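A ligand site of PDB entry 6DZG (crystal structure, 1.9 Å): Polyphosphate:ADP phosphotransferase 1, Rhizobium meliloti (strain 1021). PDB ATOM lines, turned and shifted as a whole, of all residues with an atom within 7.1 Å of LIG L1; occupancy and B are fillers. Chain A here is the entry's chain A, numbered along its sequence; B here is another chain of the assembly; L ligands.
Merely in contact with LIG L1: Ala 94 and Ala 95. Along chain A the residues within 4 Å of LIG L1 span positions 94 to 218.
The guanidinium group (NH2) of Arg 209 is in salt-bridge range of an oxygen (O1) of LIG L1, at 2.8 Å. N of Gly 98 is in hydrogen-bond range of O5 of LIG L1 (2.8 Å). N of Gly 99 is in hydrogen-bond range of O5 of LIG L1 (2.9 Å). O2 of LIG L1 lies within hydrogen-bond range of N of Lys 97 (3.0 Å). The side-chain amino group (NZ) of Lys 97 is in salt-bridge range of an oxygen (O2) of LIG L1, 3.8 Å away. An oxygen (O4) of LIG L1 lies within salt-bridge range of the side-chain amino group of Lys 218, at 3.0 Å. O1 of LIG L1 sits at hydrogen-bond distance from N of Gly 96 (3.0 Å). An oxygen (O2) of LG2 L2 is in salt-bridge range of the side-chain amino group of Lys 97, at 3.6 Å. NE of Arg 149 is in salt-bridge range of O2 of LG2 L2, at 3.3 Å. The guanidinium group (NE) of Arg 111 of chain B lies within salt-bridge range of an oxygen (O3) of LG2 L2, 2.9 Å away.
NZ of Lys 97 lies within salt-bridge range of OD1 of Asp 148 (3.1 Å). The backbone carbonyl oxygen (O) of Ala 94 is in hydrogen-bond range of the guanidinium group (NH1) of Arg 205, 2.9 Å away. NH1 of Arg 205 sits at hydrogen-bond distance from O of Ala 95 (3.1 Å).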
ATOM      1  N   ARG A  92      20.678  26.647 -26.971  1.00  0.00           N
ATOM      2  CA  ARG A  92      21.674  25.601 -27.151  1.00  0.00           C
ATOM      3  C   ARG A  92      22.784  25.771 -26.124  1.00  0.00           C
ATOM      4  O   ARG A  92      23.134  26.880 -25.743  1.00  0.00           O
ATOM      5  CB  ARG A  92      22.285  25.673 -28.559  1.00  0.00           C
ATOM      6  CG  ARG A  92      21.310  25.432 -29.666  1.00  0.00           C
ATOM      7  CD  ARG A  92      21.017  23.954 -29.779  1.00  0.00           C
ATOM      8  NE  ARG A  92      20.253  23.638 -30.971  1.00  0.00           N
ATOM      9  CZ  ARG A  92      19.915  22.404 -31.331  1.00  0.00           C
ATOM     10  NH1 ARG A  92      20.303  21.376 -30.587  1.00  0.00           N
ATOM     11  NH2 ARG A  92      19.224  22.208 -32.443  1.00  0.00           N
ATOM     12  N   ASP A  93      23.346  24.649 -25.694  1.00  0.00           N
ATOM     13  CA  ASP A  93      24.471  24.763 -24.773  1.00  0.00           C
ATOM     14  C   ASP A  93      25.599  25.510 -25.463  1.00  0.00           C
ATOM     15  O   ASP A  93      25.827  25.340 -26.667  1.00  0.00           O
ATOM     16  CB  ASP A  93      24.894  23.388 -24.295  1.00  0.00           C
ATOM     17  CG  ASP A  93      23.869  22.768 -23.329  1.00  0.00           C
ATOM     18  OD1 ASP A  93      23.428  23.460 -22.416  1.00  0.00           O
ATOM     19  OD2 ASP A  93      23.486  21.590 -23.511  1.00  0.00           O
ATOM     20  N   ALA A  94      26.259  26.394 -24.718  1.00  0.00           N
ATOM     21  CA  ALA A  94      27.316  27.269 -25.201  1.00  0.00           C
ATOM     22  C   ALA A  94      26.820  28.383 -26.120  1.00  0.00           C
ATOM     23  O   ALA A  94      27.629  29.046 -26.793  1.00  0.00           O
ATOM     24  CB  ALA A  94      28.424  26.472 -25.911  1.00  0.00           C
ATOM     25  N   ALA A  95      25.513  28.676 -26.144  1.00  0.00           N
ATOM     26  CA  ALA A  95      25.028  29.749 -27.011  1.00  0.00           C
ATOM     27  C   ALA A  95      25.293  31.143 -26.432  1.00  0.00           C
ATOM     28  O   ALA A  95      25.101  32.134 -27.139  1.00  0.00           O
ATOM     29  CB  ALA A  95      23.530  29.592 -27.287  1.00  0.00           C
ATOM     30  N   GLY A  96      25.756  31.235 -25.193  1.00  0.00           N
ATOM     31  CA  GLY A  96      26.116  32.520 -24.635  1.00  0.00           C
ATOM     32  C   GLY A  96      25.046  33.219 -23.822  1.00  0.00           C
ATOM     33  O   GLY A  96      24.976  34.451 -23.835  1.00  0.00           O
ATOM     34  N   LYS A  97      24.212  32.491 -23.086  1.00  0.00           N
ATOM     35  CA  LYS A  97      23.181  33.186 -22.325  1.00  0.00           C
ATOM     36  C   LYS A  97      23.772  34.008 -21.192  1.00  0.00           C
ATOM     37  O   LYS A  97      23.244  35.083 -20.871  1.00  0.00           O
ATOM     38  CB  LYS A  97      22.122  32.208 -21.810  1.00  0.00           C
ATOM     39  CG  LYS A  97      22.644  30.877 -21.352  1.00  0.00           C
ATOM     40  CD  LYS A  97      21.504  29.916 -21.071  1.00  0.00           C
ATOM     41  CE  LYS A  97      22.040  28.547 -20.735  1.00  0.00           C
ATOM     42  NZ  LYS A  97      23.007  28.580 -19.588  1.00  0.00           N
ATOM     43  N   GLY A  98      24.866  33.563 -20.568  1.00  0.00           N
ATOM     44  CA  GLY A  98      25.482  34.386 -19.544  1.00  0.00           C
ATOM     45  C   GLY A  98      26.053  35.677 -20.103  1.00  0.00           C
ATOM     46  O   GLY A  98      25.963  36.741 -19.478  1.00  0.00           O
ATOM     47  N   GLY A  99      26.608  35.602 -21.307  1.00  0.00           N
ATOM     48  CA  GLY A  99      27.096  36.807 -21.954  1.00  0.00           C
ATOM     49  C   GLY A  99      25.991  37.806 -22.239  1.00  0.00           C
ATOM     50  O   GLY A  99      26.193  39.024 -22.110  1.00  0.00           O
ATOM     51  N   ALA A 100      24.812  37.314 -22.654  1.00  0.00           N
ATOM     52  CA  ALA A 100      23.699  38.243 -22.850  1.00  0.00           C
ATOM     53  C   ALA A 100      23.255  38.827 -21.521  1.00  0.00           C
ATOM     54  O   ALA A 100      22.878  40.000 -21.449  1.00  0.00           O
ATOM     55  CB  ALA A 100      22.532  37.533 -23.543  1.00  0.00           C
ATOM     56  N   ILE A 101      23.317  38.032 -20.446  1.00  0.00           N
ATOM     57  CA  ILE A 101      22.943  38.553 -19.134  1.00  0.00           C
ATOM     58  C   ILE A 101      23.959  39.589 -18.652  1.00  0.00           C
ATOM     59  O   ILE A 101      23.574  40.661 -18.161  1.00  0.00           O
ATOM     60  CB  ILE A 101      22.749  37.411 -18.123  1.00  0.00           C
ATOM     61  CG1 ILE A 101      21.450  36.655 -18.437  1.00  0.00           C
ATOM     62  CG2 ILE A 101      22.770  37.947 -16.681  1.00  0.00           C
ATOM     63  CD1 ILE A 101      21.468  35.148 -18.062  1.00  0.00           C
ATOM     64  N   ASP A 148      19.208  32.728 -15.707  1.00  0.00           N
ATOM     65  CA  ASP A 148      20.250  31.991 -16.417  1.00  0.00           C
ATOM     66  C   ASP A 148      19.850  30.517 -16.340  1.00  0.00           C
ATOM     67  O   ASP A 148      20.272  29.785 -15.432  1.00  0.00           O
ATOM     68  CB  ASP A 148      21.605  32.285 -15.793  1.00  0.00           C
ATOM     69  CG  ASP A 148      22.725  31.402 -16.346  1.00  0.00           C
ATOM     70  OD1 ASP A 148      22.512  30.669 -17.343  1.00  0.00           O
ATOM     71  OD2 ASP A 148      23.829  31.439 -15.760  1.00  0.00           O
ATOM     72  N   ARG A 149      19.047  30.098 -17.322  1.00  0.00           N
ATOM     73  CA  ARG A 149      18.206  28.883 -17.301  1.00  0.00           C
ATOM     74  C   ARG A 149      17.019  29.121 -16.359  1.00  0.00           C
ATOM     75  O   ARG A 149      17.017  30.063 -15.563  1.00  0.00           O
ATOM     76  CB  ARG A 149      18.986  27.634 -16.883  1.00  0.00           C
ATOM     77  CG  ARG A 149      19.982  27.126 -17.921  1.00  0.00           C
ATOM     78  CD  ARG A 149      20.632  25.868 -17.430  1.00  0.00           C
ATOM     79  NE  ARG A 149      21.719  25.480 -18.307  1.00  0.00           N
ATOM     80  CZ  ARG A 149      21.594  24.638 -19.332  1.00  0.00           C
ATOM     81  NH1 ARG A 149      20.427  24.073 -19.593  1.00  0.00           N
ATOM     82  NH2 ARG A 149      22.661  24.341 -20.075  1.00  0.00           N
ATOM     83  N   ILE A 195      18.373  31.335 -27.492  1.00  0.00           N
ATOM     84  CA  ILE A 195      19.555  31.655 -28.299  1.00  0.00           C
ATOM     85  C   ILE A 195      20.026  30.366 -28.970  1.00  0.00           C
ATOM     86  O   ILE A 195      20.474  29.430 -28.299  1.00  0.00           O
ATOM     87  CB  ILE A 195      20.673  32.286 -27.462  1.00  0.00           C
ATOM     88  CG1 ILE A 195      20.115  33.375 -26.534  1.00  0.00           C
ATOM     89  CG2 ILE A 195      21.772  32.841 -28.377  1.00  0.00           C
ATOM     90  CD1 ILE A 195      21.148  33.959 -25.619  1.00  0.00           C
ATOM     91  N   ARG A 205      32.832  26.295 -29.838  1.00  0.00           N
ATOM     92  CA  ARG A 205      32.784  26.960 -28.530  1.00  0.00           C
ATOM     93  C   ARG A 205      33.131  25.994 -27.386  1.00  0.00           C
ATOM     94  O   ARG A 205      33.873  26.358 -26.477  1.00  0.00           O
ATOM     95  CB  ARG A 205      31.405  27.598 -28.335  1.00  0.00           C
ATOM     96  CG  ARG A 205      31.251  28.956 -29.035  1.00  0.00           C
ATOM     97  CD  ARG A 205      29.862  29.543 -28.850  1.00  0.00           C
ATOM     98  NE  ARG A 205      29.594  30.630 -29.793  1.00  0.00           N
ATOM     99  CZ  ARG A 205      28.499  31.393 -29.756  1.00  0.00           C
ATOM    100  NH1 ARG A 205      27.573  31.180 -28.822  1.00  0.00           N
ATOM    101  NH2 ARG A 205      28.301  32.363 -30.651  1.00  0.00           N
ATOM    102  N   ARG A 209      36.387  26.709 -25.070  1.00  0.00           N
ATOM    103  CA  ARG A 209      36.288  26.747 -23.619  1.00  0.00           C
ATOM    104  C   ARG A 209      37.210  25.722 -22.980  1.00  0.00           C
ATOM    105  O   ARG A 209      37.874  26.026 -21.984  1.00  0.00           O
ATOM    106  CB  ARG A 209      34.840  26.493 -23.210  1.00  0.00           C
ATOM    107  CG  ARG A 209      33.967  27.660 -23.623  1.00  0.00           C
ATOM    108  CD  ARG A 209      32.491  27.380 -23.506  1.00  0.00           C
ATOM    109  NE  ARG A 209      31.763  28.579 -23.911  1.00  0.00           N
ATOM    110  CZ  ARG A 209      30.485  28.810 -23.642  1.00  0.00           C
ATOM    111  NH1 ARG A 209      29.755  27.930 -22.960  1.00  0.00           N
ATOM    112  NH2 ARG A 209      29.932  29.943 -24.055  1.00  0.00           N
ATOM    113  N   LYS A 215      38.255  30.101 -19.372  1.00  0.00           N
ATOM    114  CA  LYS A 215      36.873  29.785 -19.697  1.00  0.00           C
ATOM    115  C   LYS A 215      36.529  28.311 -19.492  1.00  0.00           C
ATOM    116  O   LYS A 215      35.385  27.925 -19.759  1.00  0.00           O
ATOM    117  CB  LYS A 215      36.578  30.164 -21.159  1.00  0.00           C
ATOM    118  CG  LYS A 215      36.885  31.596 -21.519  1.00  0.00           C
ATOM    119  CD  LYS A 215      36.058  32.561 -20.730  1.00  0.00           C
ATOM    120  CE  LYS A 215      36.426  33.996 -21.067  1.00  0.00           C
ATOM    121  NZ  LYS A 215      36.658  34.129 -22.533  1.00  0.00           N
ATOM    122  N   TRP A 217      35.899  26.845 -16.883  1.00  0.00           N
ATOM    123  CA  TRP A 217      34.796  26.730 -15.929  1.00  0.00           C
ATOM    124  C   TRP A 217      33.452  26.615 -16.633  1.00  0.00           C
ATOM    125  O   TRP A 217      32.522  25.986 -16.115  1.00  0.00           O
ATOM    126  CB  TRP A 217      34.778  27.921 -14.957  1.00  0.00           C
ATOM    127  CG  TRP A 217      34.541  29.248 -15.612  1.00  0.00           C
ATOM    128  CD1 TRP A 217      35.488  30.093 -16.122  1.00  0.00           C
ATOM    129  CD2 TRP A 217      33.272  29.892 -15.823  1.00  0.00           C
ATOM    130  NE1 TRP A 217      34.881  31.221 -16.651  1.00  0.00           N
ATOM    131  CE2 TRP A 217      33.520  31.120 -16.477  1.00  0.00           C
ATOM    132  CE3 TRP A 217      31.938  29.537 -15.540  1.00  0.00           C
ATOM    133  CZ2 TRP A 217      32.503  32.016 -16.833  1.00  0.00           C
ATOM    134  CZ3 TRP A 217      30.928  30.434 -15.889  1.00  0.00           C
ATOM    135  CH2 TRP A 217      31.217  31.647 -16.539  1.00  0.00           C
ATOM    136  N   LYS A 218      33.342  27.178 -17.839  1.00  0.00           N
ATOM    137  CA  LYS A 218      32.093  27.161 -18.581  1.00  0.00           C
ATOM    138  C   LYS A 218      31.698  25.770 -19.059  1.00  0.00           C
ATOM    139  O   LYS A 218      30.562  25.598 -19.522  1.00  0.00           O
ATOM    140  CB  LYS A 218      32.185  28.104 -19.788  1.00  0.00           C
ATOM    141  CG  LYS A 218      32.261  29.589 -19.418  1.00  0.00           C
ATOM    142  CD  LYS A 218      32.326  30.443 -20.684  1.00  0.00           C
ATOM    143  CE  LYS A 218      32.293  31.928 -20.376  1.00  0.00           C
ATOM    144  NZ  LYS A 218      32.383  32.710 -21.642  1.00  0.00           N
ATOM    145  N   ARG A 263      23.813  39.706 -28.387  1.00  0.00           N
ATOM    146  CA  ARG A 263      23.609  40.552 -27.220  1.00  0.00           C
ATOM    147  C   ARG A 263      22.894  41.852 -27.582  1.00  0.00           C
ATOM    148  O   ARG A 263      21.998  42.296 -26.860  1.00  0.00           O
ATOM    149  CB  ARG A 263      24.957  40.857 -26.576  1.00  0.00           C
ATOM    150  CG  ARG A 263      25.715  39.611 -26.109  1.00  0.00           C
ATOM    151  CD  ARG A 263      27.122  39.968 -25.674  1.00  0.00           C
ATOM    152  NE  ARG A 263      27.870  38.777 -25.261  1.00  0.00           N
ATOM    153  CZ  ARG A 263      29.195  38.730 -25.151  1.00  0.00           C
ATOM    154  NH1 ARG A 263      29.915  39.806 -25.443  1.00  0.00           N
ATOM    155  NH2 ARG A 263      29.790  37.598 -24.766  1.00  0.00           N
ATOM    156  N   PRO B 110      28.228  31.384 -12.126  1.00  0.00           N
ATOM    157  CA  PRO B 110      27.189  32.058 -11.326  1.00  0.00           C
ATOM    158  C   PRO B 110      26.357  31.092 -10.472  1.00  0.00           C
ATOM    159  O   PRO B 110      25.620  31.565  -9.601  1.00  0.00           O
ATOM    160  CB  PRO B 110      26.326  32.743 -12.384  1.00  0.00           C
ATOM    161  CG  PRO B 110      26.562  31.971 -13.649  1.00  0.00           C
ATOM    162  CD  PRO B 110      28.000  31.524 -13.577  1.00  0.00           C
ATOM    163  N   ARG B 111      26.461  29.784 -10.665  1.00  0.00           N
ATOM    164  CA  ARG B 111      25.720  28.859  -9.808  1.00  0.00           C
ATOM    165  C   ARG B 111      26.460  28.537  -8.526  1.00  0.00           C
ATOM    166  O   ARG B 111      25.864  27.929  -7.634  1.00  0.00           O
ATOM    167  CB  ARG B 111      25.389  27.564 -10.562  1.00  0.00           C
ATOM    168  CG  ARG B 111      24.458  27.809 -11.756  1.00  0.00           C
ATOM    169  CD  ARG B 111      23.923  26.564 -12.443  1.00  0.00           C
ATOM    170  NE  ARG B 111      23.600  26.938 -13.820  1.00  0.00           N
ATOM    171  CZ  ARG B 111      22.500  27.590 -14.186  1.00  0.00           C
ATOM    172  NH1 ARG B 111      21.576  27.884 -13.272  1.00  0.00           N
ATOM    173  NH2 ARG B 111      22.331  27.948 -15.459  1.00  0.00           N
HETATM  174  C1  LIG L   1      26.557  29.959 -22.076  1.00  0.00           C
HETATM  175  O1  LIG L   1      27.332  29.792 -23.030  1.00  0.00           O
HETATM  176  O2  LIG L   1      25.339  29.876 -22.315  1.00  0.00           O
HETATM  177  C2  LIG L   1      27.071  30.272 -20.678  1.00  0.00           C
HETATM  178  O3  LIG L   1      26.140  31.024 -19.939  1.00  0.00           O
HETATM  179  C3  LIG L   1      28.420  30.996 -20.678  1.00  0.00           C
HETATM  180  C4  LIG L   1      28.374  32.359 -21.329  1.00  0.00           C
HETATM  181  O4  LIG L   1      29.402  33.076 -21.434  1.00  0.00           O
HETATM  182  O5  LIG L   1      27.298  32.792 -21.785  1.00  0.00           O
HETATM  183  P1  LG2 L   2      25.640  25.988 -16.264  1.00  0.00           P
HETATM  184  O1  LG2 L   2      26.792  25.619 -17.181  1.00  0.00           O
HETATM  185  O2  LG2 L   2      24.542  26.522 -17.067  1.00  0.00           O
HETATM  186  O3  LG2 L   2      26.101  27.039 -15.320  1.00  0.00           O
HETATM  187  P2  LG2 L   2      25.522  23.122 -15.751  1.00  0.00           P
HETATM  188  O4  LG2 L   2      26.143  22.980 -17.109  1.00  0.00           O
HETATM  189  O5  LG2 L   2      26.448  22.579 -14.649  1.00  0.00           O
HETATM  190  O6  LG2 L   2      25.139  24.708 -15.438  1.00  0.00           O
HETATM  191  O7  LG2 L   2      24.106  22.199 -15.755  1.00  0.00           O
HETATM  192  C1  LG2 L   2      23.118  22.574 -16.729  1.00  0.00           C
HETATM  193  C2  LG2 L   2      21.730  22.511 -16.053  1.00  0.00           C
HETATM  194  O8  LG2 L   2      21.415  21.137 -15.693  1.00  0.00           O
HETATM  195  C3  LG2 L   2      21.769  23.260 -14.703  1.00  0.00           C
HETATM  196  O9  LG2 L   2      20.571  24.036 -14.579  1.00  0.00           O
HETATM  197  C4  LG2 L   2      21.754  22.062 -13.719  1.00  0.00           C
HETATM  198  O10 LG2 L   2      21.149  22.475 -12.416  1.00  0.00           O
HETATM  199  C5  LG2 L   2      21.072  21.113 -14.317  1.00  0.00           C
HETATM  200  N1  LG2 L   2      21.379  19.830 -13.724  1.00  0.00           N
HETATM  201  C6  LG2 L   2      22.602  19.280 -13.594  1.00  0.00           C
HETATM  202  N2  LG2 L   2      22.504  18.091 -12.967  1.00  0.00           N
HETATM  203  C7  LG2 L   2      21.205  17.867 -12.710  1.00  0.00           C
HETATM  204  C8  LG2 L   2      20.545  16.844 -12.088  1.00  0.00           C
HETATM  205  N3  LG2 L   2      21.308  15.703 -11.599  1.00  0.00           N
HETATM  206  N4  LG2 L   2      19.224  16.894 -11.948  1.00  0.00           N
HETATM  207  C9  LG2 L   2      18.518  17.958 -12.411  1.00  0.00           C
HETATM  208  N5  LG2 L   2      19.149  18.990 -13.034  1.00  0.00           N
HETATM  209  C10 LG2 L   2      20.489  18.966 -13.182  1.00  0.00           C
